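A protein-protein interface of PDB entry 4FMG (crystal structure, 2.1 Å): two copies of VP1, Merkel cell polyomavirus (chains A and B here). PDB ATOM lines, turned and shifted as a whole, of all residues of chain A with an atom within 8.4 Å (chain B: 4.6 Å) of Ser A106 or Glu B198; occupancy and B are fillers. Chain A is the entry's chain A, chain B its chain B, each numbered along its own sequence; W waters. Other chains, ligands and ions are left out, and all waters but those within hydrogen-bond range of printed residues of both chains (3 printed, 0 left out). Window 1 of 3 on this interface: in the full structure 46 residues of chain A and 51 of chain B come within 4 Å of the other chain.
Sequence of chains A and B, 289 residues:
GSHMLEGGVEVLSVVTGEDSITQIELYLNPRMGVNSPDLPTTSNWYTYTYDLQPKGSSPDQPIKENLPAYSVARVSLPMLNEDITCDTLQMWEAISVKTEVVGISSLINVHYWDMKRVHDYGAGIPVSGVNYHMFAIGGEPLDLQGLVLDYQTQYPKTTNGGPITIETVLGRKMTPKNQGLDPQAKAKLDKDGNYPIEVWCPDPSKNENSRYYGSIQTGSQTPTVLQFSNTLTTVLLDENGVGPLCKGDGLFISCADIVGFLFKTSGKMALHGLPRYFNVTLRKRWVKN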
ATOM      1  N   THR A  47      -2.986   3.933  15.947  1.00  0.00           N
ATOM      2  CA  THR A  47      -4.045   4.414  16.878  1.00  0.00           C
ATOM      3  C   THR A  47      -3.910   3.881  18.322  1.00  0.00           C
ATOM      4  O   THR A  47      -4.803   4.089  19.166  1.00  0.00           O
ATOM      5  CB  THR A  47      -5.511   4.277  16.341  1.00  0.00           C
ATOM      6  OG1 THR A  47      -5.999   2.939  16.533  1.00  0.00           O
ATOM      7  CG2 THR A  47      -5.601   4.675  14.863  1.00  0.00           C
ATOM      8  N   TYR A  48      -2.788   3.219  18.599  1.00  0.00           N
ATOM      9  CA  TYR A  48      -2.466   2.745  19.954  1.00  0.00           C
ATOM     10  C   TYR A  48      -1.074   3.194  20.382  1.00  0.00           C
ATOM     11  O   TYR A  48      -0.256   3.641  19.557  1.00  0.00           O
ATOM     12  CB  TYR A  48      -2.544   1.211  20.045  1.00  0.00           C
ATOM     13  CG  TYR A  48      -3.909   0.630  19.765  1.00  0.00           C
ATOM     14  CD1 TYR A  48      -4.792   0.349  20.807  1.00  0.00           C
ATOM     15  CD2 TYR A  48      -4.318   0.365  18.453  1.00  0.00           C
ATOM     16  CE1 TYR A  48      -6.049  -0.189  20.551  1.00  0.00           C
ATOM     17  CE2 TYR A  48      -5.569  -0.165  18.179  1.00  0.00           C
ATOM     18  CZ  TYR A  48      -6.433  -0.440  19.227  1.00  0.00           C
ATOM     19  OH  TYR A  48      -7.674  -0.968  18.955  1.00  0.00           O
ATOM     20  N   VAL A 102     -15.007  10.307  15.833  1.00  0.00           N
ATOM     21  CA  VAL A 102     -15.431   9.304  14.856  1.00  0.00           C
ATOM     22  C   VAL A 102     -15.028   7.890  15.279  1.00  0.00           C
ATOM     23  O   VAL A 102     -13.962   7.687  15.865  1.00  0.00           O
ATOM     24  CB  VAL A 102     -14.864   9.653  13.470  1.00  0.00           C
ATOM     25  CG1 VAL A 102     -15.167   8.556  12.431  1.00  0.00           C
ATOM     26  CG2 VAL A 102     -15.429  10.993  13.020  1.00  0.00           C
ATOM     27  N   GLY A 103     -15.894   6.921  14.995  1.00  0.00           N
ATOM     28  CA  GLY A 103     -15.600   5.517  15.287  1.00  0.00           C
ATOM     29  C   GLY A 103     -15.886   5.126  16.731  1.00  0.00           C
ATOM     30  O   GLY A 103     -15.410   4.090  17.210  1.00  0.00           O
ATOM     31  N   ILE A 104     -16.662   5.951  17.428  1.00  0.00           N
ATOM     32  CA  ILE A 104     -17.039   5.654  18.805  1.00  0.00           C
ATOM     33  C   ILE A 104     -17.609   4.232  18.934  1.00  0.00           C
ATOM     34  O   ILE A 104     -17.244   3.488  19.853  1.00  0.00           O
ATOM     35  CB  ILE A 104     -18.008   6.718  19.372  1.00  0.00           C
ATOM     36  CG1 ILE A 104     -17.242   8.007  19.687  1.00  0.00           C
ATOM     37  CG2 ILE A 104     -18.703   6.200  20.606  1.00  0.00           C
ATOM     38  CD1 ILE A 104     -18.131   9.216  20.002  1.00  0.00           C
ATOM     39  N   SER A 105     -18.468   3.859  17.986  1.00  0.00           N
ATOM     40  CA  SER A 105     -19.114   2.541  17.958  1.00  0.00           C
ATOM     41  C   SER A 105     -18.140   1.350  17.915  1.00  0.00           C
ATOM     42  O   SER A 105     -18.490   0.249  18.339  1.00  0.00           O
ATOM     43  CB  SER A 105     -20.087   2.453  16.776  1.00  0.00           C
ATOM     44  OG  SER A 105     -19.386   2.360  15.541  1.00  0.00           O
ATOM     45  N   SER A 106     -16.930   1.575  17.407  1.00  0.00           N
ATOM     46  CA  SER A 106     -15.914   0.526  17.320  1.00  0.00           C
ATOM     47  C   SER A 106     -15.560  -0.026  18.701  1.00  0.00           C
ATOM     48  O   SER A 106     -15.053  -1.145  18.814  1.00  0.00           O
ATOM     49  CB  SER A 106     -14.651   1.056  16.652  1.00  0.00           C
ATOM     50  OG  SER A 106     -13.968   1.934  17.535  1.00  0.00           O
ATOM     51  N   LEU A 107     -15.844   0.762  19.739  1.00  0.00           N
ATOM     52  CA  LEU A 107     -15.534   0.393  21.113  1.00  0.00           C
ATOM     53  C   LEU A 107     -16.530  -0.549  21.796  1.00  0.00           C
ATOM     54  O   LEU A 107     -16.339  -0.890  22.966  1.00  0.00           O
ATOM     55  CB  LEU A 107     -15.285   1.643  21.979  1.00  0.00           C
ATOM     56  CG  LEU A 107     -14.350   2.746  21.462  1.00  0.00           C
ATOM     57  CD1 LEU A 107     -14.296   3.895  22.463  1.00  0.00           C
ATOM     58  CD2 LEU A 107     -12.943   2.219  21.159  1.00  0.00           C
ATOM     59  N   ILE A 108     -17.580  -0.991  21.106  1.00  0.00           N
ATOM     60  CA  ILE A 108     -18.421  -2.059  21.689  1.00  0.00           C
ATOM     61  C   ILE A 108     -17.778  -3.450  21.570  1.00  0.00           C
ATOM     62  O   ILE A 108     -18.283  -4.418  22.156  1.00  0.00           O
ATOM     63  CB  ILE A 108     -19.878  -2.116  21.142  1.00  0.00           C
ATOM     64  CG1 ILE A 108     -19.916  -2.648  19.705  1.00  0.00           C
ATOM     65  CG2 ILE A 108     -20.583  -0.765  21.277  1.00  0.00           C
ATOM     66  CD1 ILE A 108     -21.208  -3.342  19.362  1.00  0.00           C
ATOM     67  N   ASN A 109     -16.680  -3.541  20.812  1.00  0.00           N
ATOM     68  CA  ASN A 109     -15.968  -4.801  20.602  1.00  0.00           C
ATOM     69  C   ASN A 109     -15.309  -5.293  21.899  1.00  0.00           C
ATOM     70  O   ASN A 109     -14.355  -4.685  22.397  1.00  0.00           O
ATOM     71  CB  ASN A 109     -14.934  -4.647  19.472  1.00  0.00           C
ATOM     72  CG  ASN A 109     -14.199  -5.958  19.135  1.00  0.00           C
ATOM     73  OD1 ASN A 109     -14.241  -6.935  19.881  1.00  0.00           O
ATOM     74  ND2 ASN A 109     -13.515  -5.965  18.005  1.00  0.00           N
ATOM     75  N   VAL A 110     -15.841  -6.384  22.443  1.00  0.00           N
ATOM     76  CA  VAL A 110     -15.286  -7.030  23.637  1.00  0.00           C
ATOM     77  C   VAL A 110     -14.762  -8.430  23.305  1.00  0.00           C
ATOM     78  O   VAL A 110     -14.799  -9.341  24.142  1.00  0.00           O
ATOM     79  CB  VAL A 110     -16.310  -7.084  24.804  1.00  0.00           C
ATOM     80  CG1 VAL A 110     -16.599  -5.678  25.334  1.00  0.00           C
ATOM     81  CG2 VAL A 110     -17.594  -7.776  24.379  1.00  0.00           C
ATOM     82  N   HIS A 111     -14.276  -8.592  22.073  1.00  0.00           N
ATOM     83  CA  HIS A 111     -13.749  -9.869  21.597  1.00  0.00           C
ATOM     84  C   HIS A 111     -12.489  -9.701  20.745  1.00  0.00           C
ATOM     85  O   HIS A 111     -12.258 -10.459  19.805  1.00  0.00           O
ATOM     86  CB  HIS A 111     -14.824 -10.645  20.823  1.00  0.00           C
ATOM     87  CG  HIS A 111     -15.445  -9.856  19.714  1.00  0.00           C
ATOM     88  ND1 HIS A 111     -14.911  -9.812  18.443  1.00  0.00           N
ATOM     89  CD2 HIS A 111     -16.532  -9.050  19.696  1.00  0.00           C
ATOM     90  CE1 HIS A 111     -15.654  -9.024  17.685  1.00  0.00           C
ATOM     91  NE2 HIS A 111     -16.642  -8.547  18.423  1.00  0.00           N
ATOM     92  N   TYR A 112     -11.674  -8.699  21.070  1.00  0.00           N
ATOM     93  CA  TYR A 112     -10.323  -8.636  20.537  1.00  0.00           C
ATOM     94  C   TYR A 112      -9.670  -9.976  20.904  1.00  0.00           C
ATOM     95  O   TYR A 112      -9.871 -10.473  22.008  1.00  0.00           O
ATOM     96  CB  TYR A 112      -9.578  -7.449  21.144  1.00  0.00           C
ATOM     97  CG  TYR A 112      -8.090  -7.470  20.932  1.00  0.00           C
ATOM     98  CD1 TYR A 112      -7.547  -7.505  19.643  1.00  0.00           C
ATOM     99  CD2 TYR A 112      -7.216  -7.447  22.019  1.00  0.00           C
ATOM    100  CE1 TYR A 112      -6.173  -7.529  19.447  1.00  0.00           C
ATOM    101  CE2 TYR A 112      -5.842  -7.463  21.833  1.00  0.00           C
ATOM    102  CZ  TYR A 112      -5.326  -7.509  20.542  1.00  0.00           C
ATOM    103  OH  TYR A 112      -3.964  -7.528  20.349  1.00  0.00           O
ATOM    104  N   MET A 115      -7.699 -10.095  24.297  1.00  0.00           N
ATOM    105  CA  MET A 115      -8.255  -9.211  25.327  1.00  0.00           C
ATOM    106  C   MET A 115      -8.302  -9.938  26.668  1.00  0.00           C
ATOM    107  O   MET A 115      -8.738 -11.089  26.751  1.00  0.00           O
ATOM    108  CB  MET A 115      -9.667  -8.763  24.929  1.00  0.00           C
ATOM    109  CG  MET A 115      -9.993  -7.278  25.110  1.00  0.00           C
ATOM    110  SD  MET A 115     -11.595  -6.889  24.333  1.00  0.00           S
ATOM    111  CE  MET A 115     -11.513  -5.111  24.191  1.00  0.00           C
ATOM    112  N   VAL A 127     -12.614  -1.325  26.120  1.00  0.00           N
ATOM    113  CA  VAL A 127     -11.773  -0.134  26.165  1.00  0.00           C
ATOM    114  C   VAL A 127     -12.384   0.845  27.168  1.00  0.00           C
ATOM    115  O   VAL A 127     -13.507   1.334  26.994  1.00  0.00           O
ATOM    116  CB  VAL A 127     -11.572   0.500  24.763  1.00  0.00           C
ATOM    117  CG1 VAL A 127     -10.902   1.878  24.865  1.00  0.00           C
ATOM    118  CG2 VAL A 127     -10.738  -0.426  23.879  1.00  0.00           C
ATOM    119  N   PHE A 228     -22.266  11.541  20.362  1.00  0.00           N
ATOM    120  CA  PHE A 228     -22.103  11.930  18.964  1.00  0.00           C
ATOM    121  C   PHE A 228     -23.446  12.357  18.372  1.00  0.00           C
ATOM    122  O   PHE A 228     -24.448  11.664  18.525  1.00  0.00           O
ATOM    123  CB  PHE A 228     -21.437  10.814  18.120  1.00  0.00           C
ATOM    124  CG  PHE A 228     -22.124   9.479  18.219  1.00  0.00           C
ATOM    125  CD1 PHE A 228     -21.878   8.633  19.299  1.00  0.00           C
ATOM    126  CD2 PHE A 228     -23.009   9.064  17.232  1.00  0.00           C
ATOM    127  CE1 PHE A 228     -22.517   7.402  19.403  1.00  0.00           C
ATOM    128  CE2 PHE A 228     -23.655   7.833  17.323  1.00  0.00           C
ATOM    129  CZ  PHE A 228     -23.410   6.999  18.407  1.00  0.00           C
ATOM    130  N   VAL A 259      -9.295   7.433  24.412  1.00  0.00           N
ATOM    131  CA  VAL A 259     -10.573   6.830  24.760  1.00  0.00           C
ATOM    132  C   VAL A 259     -10.484   5.653  25.765  1.00  0.00           C
ATOM    133  O   VAL A 259     -11.487   4.994  26.054  1.00  0.00           O
ATOM    134  CB  VAL A 259     -11.373   6.436  23.471  1.00  0.00           C
ATOM    135  CG1 VAL A 259     -11.702   7.688  22.649  1.00  0.00           C
ATOM    136  CG2 VAL A 259     -10.604   5.422  22.620  1.00  0.00           C
ATOM    137  N   HIS A 272      -5.438   4.086  23.741  1.00  0.00           N
ATOM    138  CA  HIS A 272      -6.060   4.035  22.414  1.00  0.00           C
ATOM    139  C   HIS A 272      -6.701   5.378  22.118  1.00  0.00           C
ATOM    140  O   HIS A 272      -7.184   6.049  23.030  1.00  0.00           O
ATOM    141  CB  HIS A 272      -7.128   2.938  22.408  1.00  0.00           C
ATOM    142  CG  HIS A 272      -7.808   2.728  21.088  1.00  0.00           C
ATOM    143  ND1 HIS A 272      -7.152   2.834  19.876  1.00  0.00           N
ATOM    144  CD2 HIS A 272      -9.079   2.358  20.796  1.00  0.00           C
ATOM    145  CE1 HIS A 272      -7.997   2.562  18.895  1.00  0.00           C
ATOM    146  NE2 HIS A 272      -9.172   2.272  19.427  1.00  0.00           N
ATOM    147  N   GLY A 273      -6.702   5.766  20.845  1.00  0.00           N
ATOM    148  CA  GLY A 273      -7.272   7.041  20.420  1.00  0.00           C
ATOM    149  C   GLY A 273      -8.196   6.908  19.223  1.00  0.00           C
ATOM    150  O   GLY A 273      -8.079   5.949  18.444  1.00  0.00           O
ATOM    151  N   LEU A 274      -9.117   7.869  19.094  1.00  0.00           N
ATOM    152  CA  LEU A 274     -10.045   7.951  17.968  1.00  0.00           C
ATOM    153  C   LEU A 274      -9.858   9.256  17.190  1.00  0.00           C
ATOM    154  O   LEU A 274      -9.443  10.266  17.779  1.00  0.00           O
ATOM    155  CB  LEU A 274     -11.507   7.837  18.436  1.00  0.00           C
ATOM    156  CG  LEU A 274     -12.020   6.481  18.928  1.00  0.00           C
ATOM    157  CD1 LEU A 274     -13.482   6.587  19.326  1.00  0.00           C
ATOM    158  CD2 LEU A 274     -11.838   5.367  17.912  1.00  0.00           C
ATOM    159  N   PRO A 275     -10.165   9.237  15.864  1.00  0.00           N
ATOM    160  CA  PRO A 275     -10.073  10.415  14.996  1.00  0.00           C
ATOM    161  C   PRO A 275     -11.158  11.436  15.306  1.00  0.00           C
ATOM    162  O   PRO A 275     -12.185  11.104  15.908  1.00  0.00           O
ATOM    163  CB  PRO A 275     -10.306   9.848  13.588  1.00  0.00           C
ATOM    164  CG  PRO A 275     -10.283   8.363  13.734  1.00  0.00           C
ATOM    165  CD  PRO A 275     -10.696   8.078  15.128  1.00  0.00           C
ATOM    166  N   LEU B  67     -22.369 -10.129  16.441  1.00  0.00           N
ATOM    167  CA  LEU B  67     -22.216  -8.822  15.795  1.00  0.00           C
ATOM    168  C   LEU B  67     -23.527  -8.032  15.783  1.00  0.00           C
ATOM    169  O   LEU B  67     -24.245  -8.020  14.763  1.00  0.00           O
ATOM    170  CB  LEU B  67     -21.645  -8.975  14.372  1.00  0.00           C
ATOM    171  CG  LEU B  67     -20.272  -9.657  14.252  1.00  0.00           C
ATOM    172  CD1 LEU B  67     -19.894  -9.934  12.791  1.00  0.00           C
ATOM    173  CD2 LEU B  67     -19.178  -8.845  14.963  1.00  0.00           C
ATOM    174  N   LEU B 147     -14.835   2.096  10.785  1.00  0.00           N
ATOM    175  CA  LEU B 147     -13.665   2.132  11.675  1.00  0.00           C
ATOM    176  C   LEU B 147     -13.756   0.972  12.653  1.00  0.00           C
ATOM    177  O   LEU B 147     -14.781   0.784  13.314  1.00  0.00           O
ATOM    178  CB  LEU B 147     -13.576   3.460  12.441  1.00  0.00           C
ATOM    179  CG  LEU B 147     -12.296   3.789  13.220  1.00  0.00           C
ATOM    180  CD1 LEU B 147     -12.133   5.290  13.318  1.00  0.00           C
ATOM    181  CD2 LEU B 147     -12.265   3.160  14.623  1.00  0.00           C
ATOM    182  N   VAL B 148     -12.677   0.207  12.750  1.00  0.00           N
ATOM    183  CA  VAL B 148     -12.659  -0.985  13.591  1.00  0.00           C
ATOM    184  C   VAL B 148     -11.549  -0.954  14.644  1.00  0.00           C
ATOM    185  O   VAL B 148     -10.507  -0.314  14.453  1.00  0.00           O
ATOM    186  CB  VAL B 148     -12.517  -2.291  12.757  1.00  0.00           C
ATOM    187  CG1 VAL B 148     -13.716  -2.492  11.876  1.00  0.00           C
ATOM    188  CG2 VAL B 148     -11.214  -2.290  11.940  1.00  0.00           C
ATOM    189  N   LEU B 149     -11.793  -1.650  15.754  1.00  0.00           N
ATOM    190  CA  LEU B 149     -10.795  -1.818  16.810  1.00  0.00           C
ATOM    191  C   LEU B 149      -9.544  -2.498  16.242  1.00  0.00           C
ATOM    192  O   LEU B 149      -8.425  -2.020  16.429  1.00  0.00           O
ATOM    193  CB  LEU B 149     -11.381  -2.632  17.977  1.00  0.00           C
ATOM    194  CG  LEU B 149     -10.578  -2.711  19.285  1.00  0.00           C
ATOM    195  CD1 LEU B 149     -10.627  -1.402  20.085  1.00  0.00           C
ATOM    196  CD2 LEU B 149     -11.075  -3.856  20.135  1.00  0.00           C
ATOM    197  N   TYR B 155     -14.208 -10.747   9.497  1.00  0.00           N
ATOM    198  CA  TYR B 155     -15.677 -10.791   9.580  1.00  0.00           C
ATOM    199  C   TYR B 155     -16.206 -11.773   8.547  1.00  0.00           C
ATOM    200  O   TYR B 155     -15.571 -11.960   7.512  1.00  0.00           O
ATOM    201  CB  TYR B 155     -16.292  -9.395   9.391  1.00  0.00           C
ATOM    202  CG  TYR B 155     -15.938  -8.453  10.518  1.00  0.00           C
ATOM    203  CD1 TYR B 155     -16.609  -8.521  11.744  1.00  0.00           C
ATOM    204  CD2 TYR B 155     -14.911  -7.511  10.372  1.00  0.00           C
ATOM    205  CE1 TYR B 155     -16.273  -7.663  12.799  1.00  0.00           C
ATOM    206  CE2 TYR B 155     -14.571  -6.646  11.418  1.00  0.00           C
ATOM    207  CZ  TYR B 155     -15.256  -6.730  12.629  1.00  0.00           C
ATOM    208  OH  TYR B 155     -14.914  -5.894  13.670  1.00  0.00           O
ATOM    209  N   PRO B 196     -22.791  -4.009  11.064  1.00  0.00           N
ATOM    210  CA  PRO B 196     -22.348  -4.137  12.453  1.00  0.00           C
ATOM    211  C   PRO B 196     -22.020  -2.808  13.121  1.00  0.00           C
ATOM    212  O   PRO B 196     -21.337  -1.963  12.539  1.00  0.00           O
ATOM    213  CB  PRO B 196     -21.091  -5.010  12.336  1.00  0.00           C
ATOM    214  CG  PRO B 196     -21.331  -5.829  11.098  1.00  0.00           C
ATOM    215  CD  PRO B 196     -21.986  -4.849  10.156  1.00  0.00           C
ATOM    216  N   ILE B 197     -22.512  -2.649  14.347  1.00  0.00           N
ATOM    217  CA  ILE B 197     -22.239  -1.483  15.169  1.00  0.00           C
ATOM    218  C   ILE B 197     -20.735  -1.302  15.431  1.00  0.00           C
ATOM    219  O   ILE B 197     -20.240  -0.167  15.421  1.00  0.00           O
ATOM    220  CB  ILE B 197     -23.057  -1.533  16.478  1.00  0.00           C
ATOM    221  CG1 ILE B 197     -24.547  -1.323  16.171  1.00  0.00           C
ATOM    222  CG2 ILE B 197     -22.579  -0.483  17.455  1.00  0.00           C
ATOM    223  CD1 ILE B 197     -25.507  -2.154  17.039  1.00  0.00           C
ATOM    224  N   GLU B 198     -20.002  -2.404  15.622  1.00  0.00           N
ATOM    225  CA  GLU B 198     -18.559  -2.302  15.892  1.00  0.00           C
ATOM    226  C   GLU B 198     -17.718  -1.940  14.654  1.00  0.00           C
ATOM    227  O   GLU B 198     -16.520  -1.668  14.763  1.00  0.00           O
ATOM    228  CB  GLU B 198     -18.026  -3.581  16.549  1.00  0.00           C
ATOM    229  CG  GLU B 198     -17.717  -4.708  15.580  1.00  0.00           C
ATOM    230  CD  GLU B 198     -17.170  -5.941  16.280  1.00  0.00           C
ATOM    231  OE1 GLU B 198     -17.687  -6.314  17.368  1.00  0.00           O
ATOM    232  OE2 GLU B 198     -16.223  -6.538  15.728  1.00  0.00           O
ATOM    233  N   VAL B 199     -18.354  -1.934  13.483  1.00  0.00           N
ATOM    234  CA  VAL B 199     -17.675  -1.609  12.226  1.00  0.00           C
ATOM    235  C   VAL B 199     -18.060  -0.205  11.739  1.00  0.00           C
ATOM    236  O   VAL B 199     -17.211   0.555  11.256  1.00  0.00           O
ATOM    237  CB  VAL B 199     -18.010  -2.662  11.123  1.00  0.00           C
ATOM    238  CG1 VAL B 199     -17.323  -2.318   9.814  1.00  0.00           C
ATOM    239  CG2 VAL B 199     -17.617  -4.065  11.576  1.00  0.00           C
ATOM    240  N   TRP B 200     -19.339   0.136  11.892  1.00  0.00           N
ATOM    241  CA  TRP B 200     -19.901   1.327  11.264  1.00  0.00           C
ATOM    242  C   TRP B 200     -20.443   2.332  12.270  1.00  0.00           C
ATOM    243  O   TRP B 200     -21.202   1.978  13.176  1.00  0.00           O
ATOM    244  CB  TRP B 200     -21.038   0.938  10.306  1.00  0.00           C
ATOM    245  CG  TRP B 200     -20.655  -0.001   9.190  1.00  0.00           C
ATOM    246  CD1 TRP B 200     -20.990  -1.321   9.083  1.00  0.00           C
ATOM    247  CD2 TRP B 200     -19.897   0.316   8.014  1.00  0.00           C
ATOM    248  NE1 TRP B 200     -20.473  -1.847   7.924  1.00  0.00           N
ATOM    249  CE2 TRP B 200     -19.801  -0.864   7.249  1.00  0.00           C
ATOM    250  CE3 TRP B 200     -19.281   1.484   7.537  1.00  0.00           C
ATOM    251  CZ2 TRP B 200     -19.113  -0.913   6.032  1.00  0.00           C
ATOM    252  CZ3 TRP B 200     -18.596   1.432   6.335  1.00  0.00           C
ATOM    253  CH2 TRP B 200     -18.515   0.241   5.600  1.00  0.00           C
HETATM  254  O   HOH W   1     -14.609  -2.723  16.452  1.00  0.00           O
HETATM  255  O   HOH W   2     -16.995   2.872  13.972  1.00  0.00           O
HETATM  256  O   HOH W   3     -12.377  -4.730  15.139  1.00  0.00           O
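O of Leu B149 lies within hydrogen-bond range of OH of Tyr A48.
The side-chain hydroxyl (OG) of Ser A105 sits at hydrogen-bond distance from the backbone carbonyl oxygen (O) of Ile B197, at 2.7 Å.
O of Trp B200 lies within hydrogen-bond range of OG of Ser A105.
A ring nitrogen (NE2) of His A111 sits at hydrogen-bond distance from the side-chain carboxylate of Glu B198.
The backbone carbonyl oxygen of Pro A275 is in hydrogen-bond range of the backbone NH of Val A102 (2.9 Å).
O of Gly A103 is in hydrogen-bond range of OG of Ser A106.
The backbone NH of His A111 lies within hydrogen-bond range of the side-chain amide oxygen of Asn A109, 2.7 Å away.
The side-chain amide oxygen (OD1) of Asn A109 sits at hydrogen-bond distance from the backbone NH (N) of Tyr A112, 3.3 Å away.
N of Leu B147 lies within hydrogen-bond range of O of Val B199 (2.9 Å).
OH of Tyr B155 sits at hydrogen-bond distance from OE2 of Glu B198 (2.5 Å).
Among the printed residues, pairs that only touch across the chains: Ser A106 with Leu B147 (3.4 Å), Ser A106 with Glu B198 (3.4 Å), Ser A105 with Glu B198 (3.5 Å), Asn A109 with Glu B198 (3.6 Å), Pro A275 with Leu B147 (3.6 Å), Ile A108 with Ile B197 (3.7 Å), Ile A108 with Glu B198 (3.8 Å), Asn A109 with Leu B149 (3.9 Å), Val A127 with Leu B149 (3.9 Å), Val A102 with Leu B147 (3.9 Å), Leu A274 with Leu B147 (3.98 Å) and Gly A103 with Leu B147 (3.99 Å).
Ser A106 touches two residues of chain B.
Glu B198 touches five residues of chain A.
Of the printed residues of chain B, Tyr A48 touches Leu B149 (2.8 Å).
Printed residues of chain B within 4 Å of Leu A274: Leu B147.
Of the printed residues of chain A, Ile B197 touches Ser A105 (2.7 Å) and Ile A108 (3.7 Å).
Of the printed residues of chain A, Leu B147 touches Val A102 (3.9 Å), Gly A103 (3.99 Å), Ser A106 (3.4 Å), Leu A274 (3.98 Å) and Pro A275 (3.6 Å).
Tyr B155 touches none of the printed residues of chain A.
Pro B196 touches none of the printed residues of chain A.
Of the 10 printed residues of chain B, 5 touch a printed residue of chain A.
Hydrophobic or aromatic side chains of chain B within 4 Å of the printed part of chain A: Leu B147, Leu B149 and Ile B197.
Of the 21 printed residues of chain A, 11 touch a printed residue of chain B.
Printed residues of chain A that touch a printed residue of chain B: Tyr A48, Val A102, Gly A103, Ser A105, Ser A106, Ile A108, Asn A109, His A111, Val A127, Leu A274 and Pro A275.
Hydrophobic or aromatic side chains of chain A that line the printed part of chain B: Tyr A48, Ile A108, His A111, Val A127, Leu A274 and Pro A275.
Along chain A the printed residues that touch a printed residue of chain B span positions 48 to 275.
Among the printed residues, 16 pairs touch across the chains.
Among the printed residues, no Asp or Glu carboxylate lies within 4 Å of a Lys or Arg side-chain nitrogen of the other chain.
No position is printed for both chains.
Of the 16 pairs that touch across the chains among the printed residues, none has its exchanged pair printed and touching as well.
Water W1 lies within hydrogen-bond range of the backbone carbonyl oxygen (O) of Glu B198 (2.8 Å), the backbone carbonyl oxygen (O) of Ser A106 (2.9 Å) and the backbone NH (N) of Leu B149 (3.1 Å).
Water W2 lies within hydrogen-bond range of OG of Ser A105 (2.9 Å) and O of Leu B147 (3.1 Å).
Water W3 lies within hydrogen-bond range of OH of Tyr B155, N of Leu B149 and ND2 of Asn A109.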
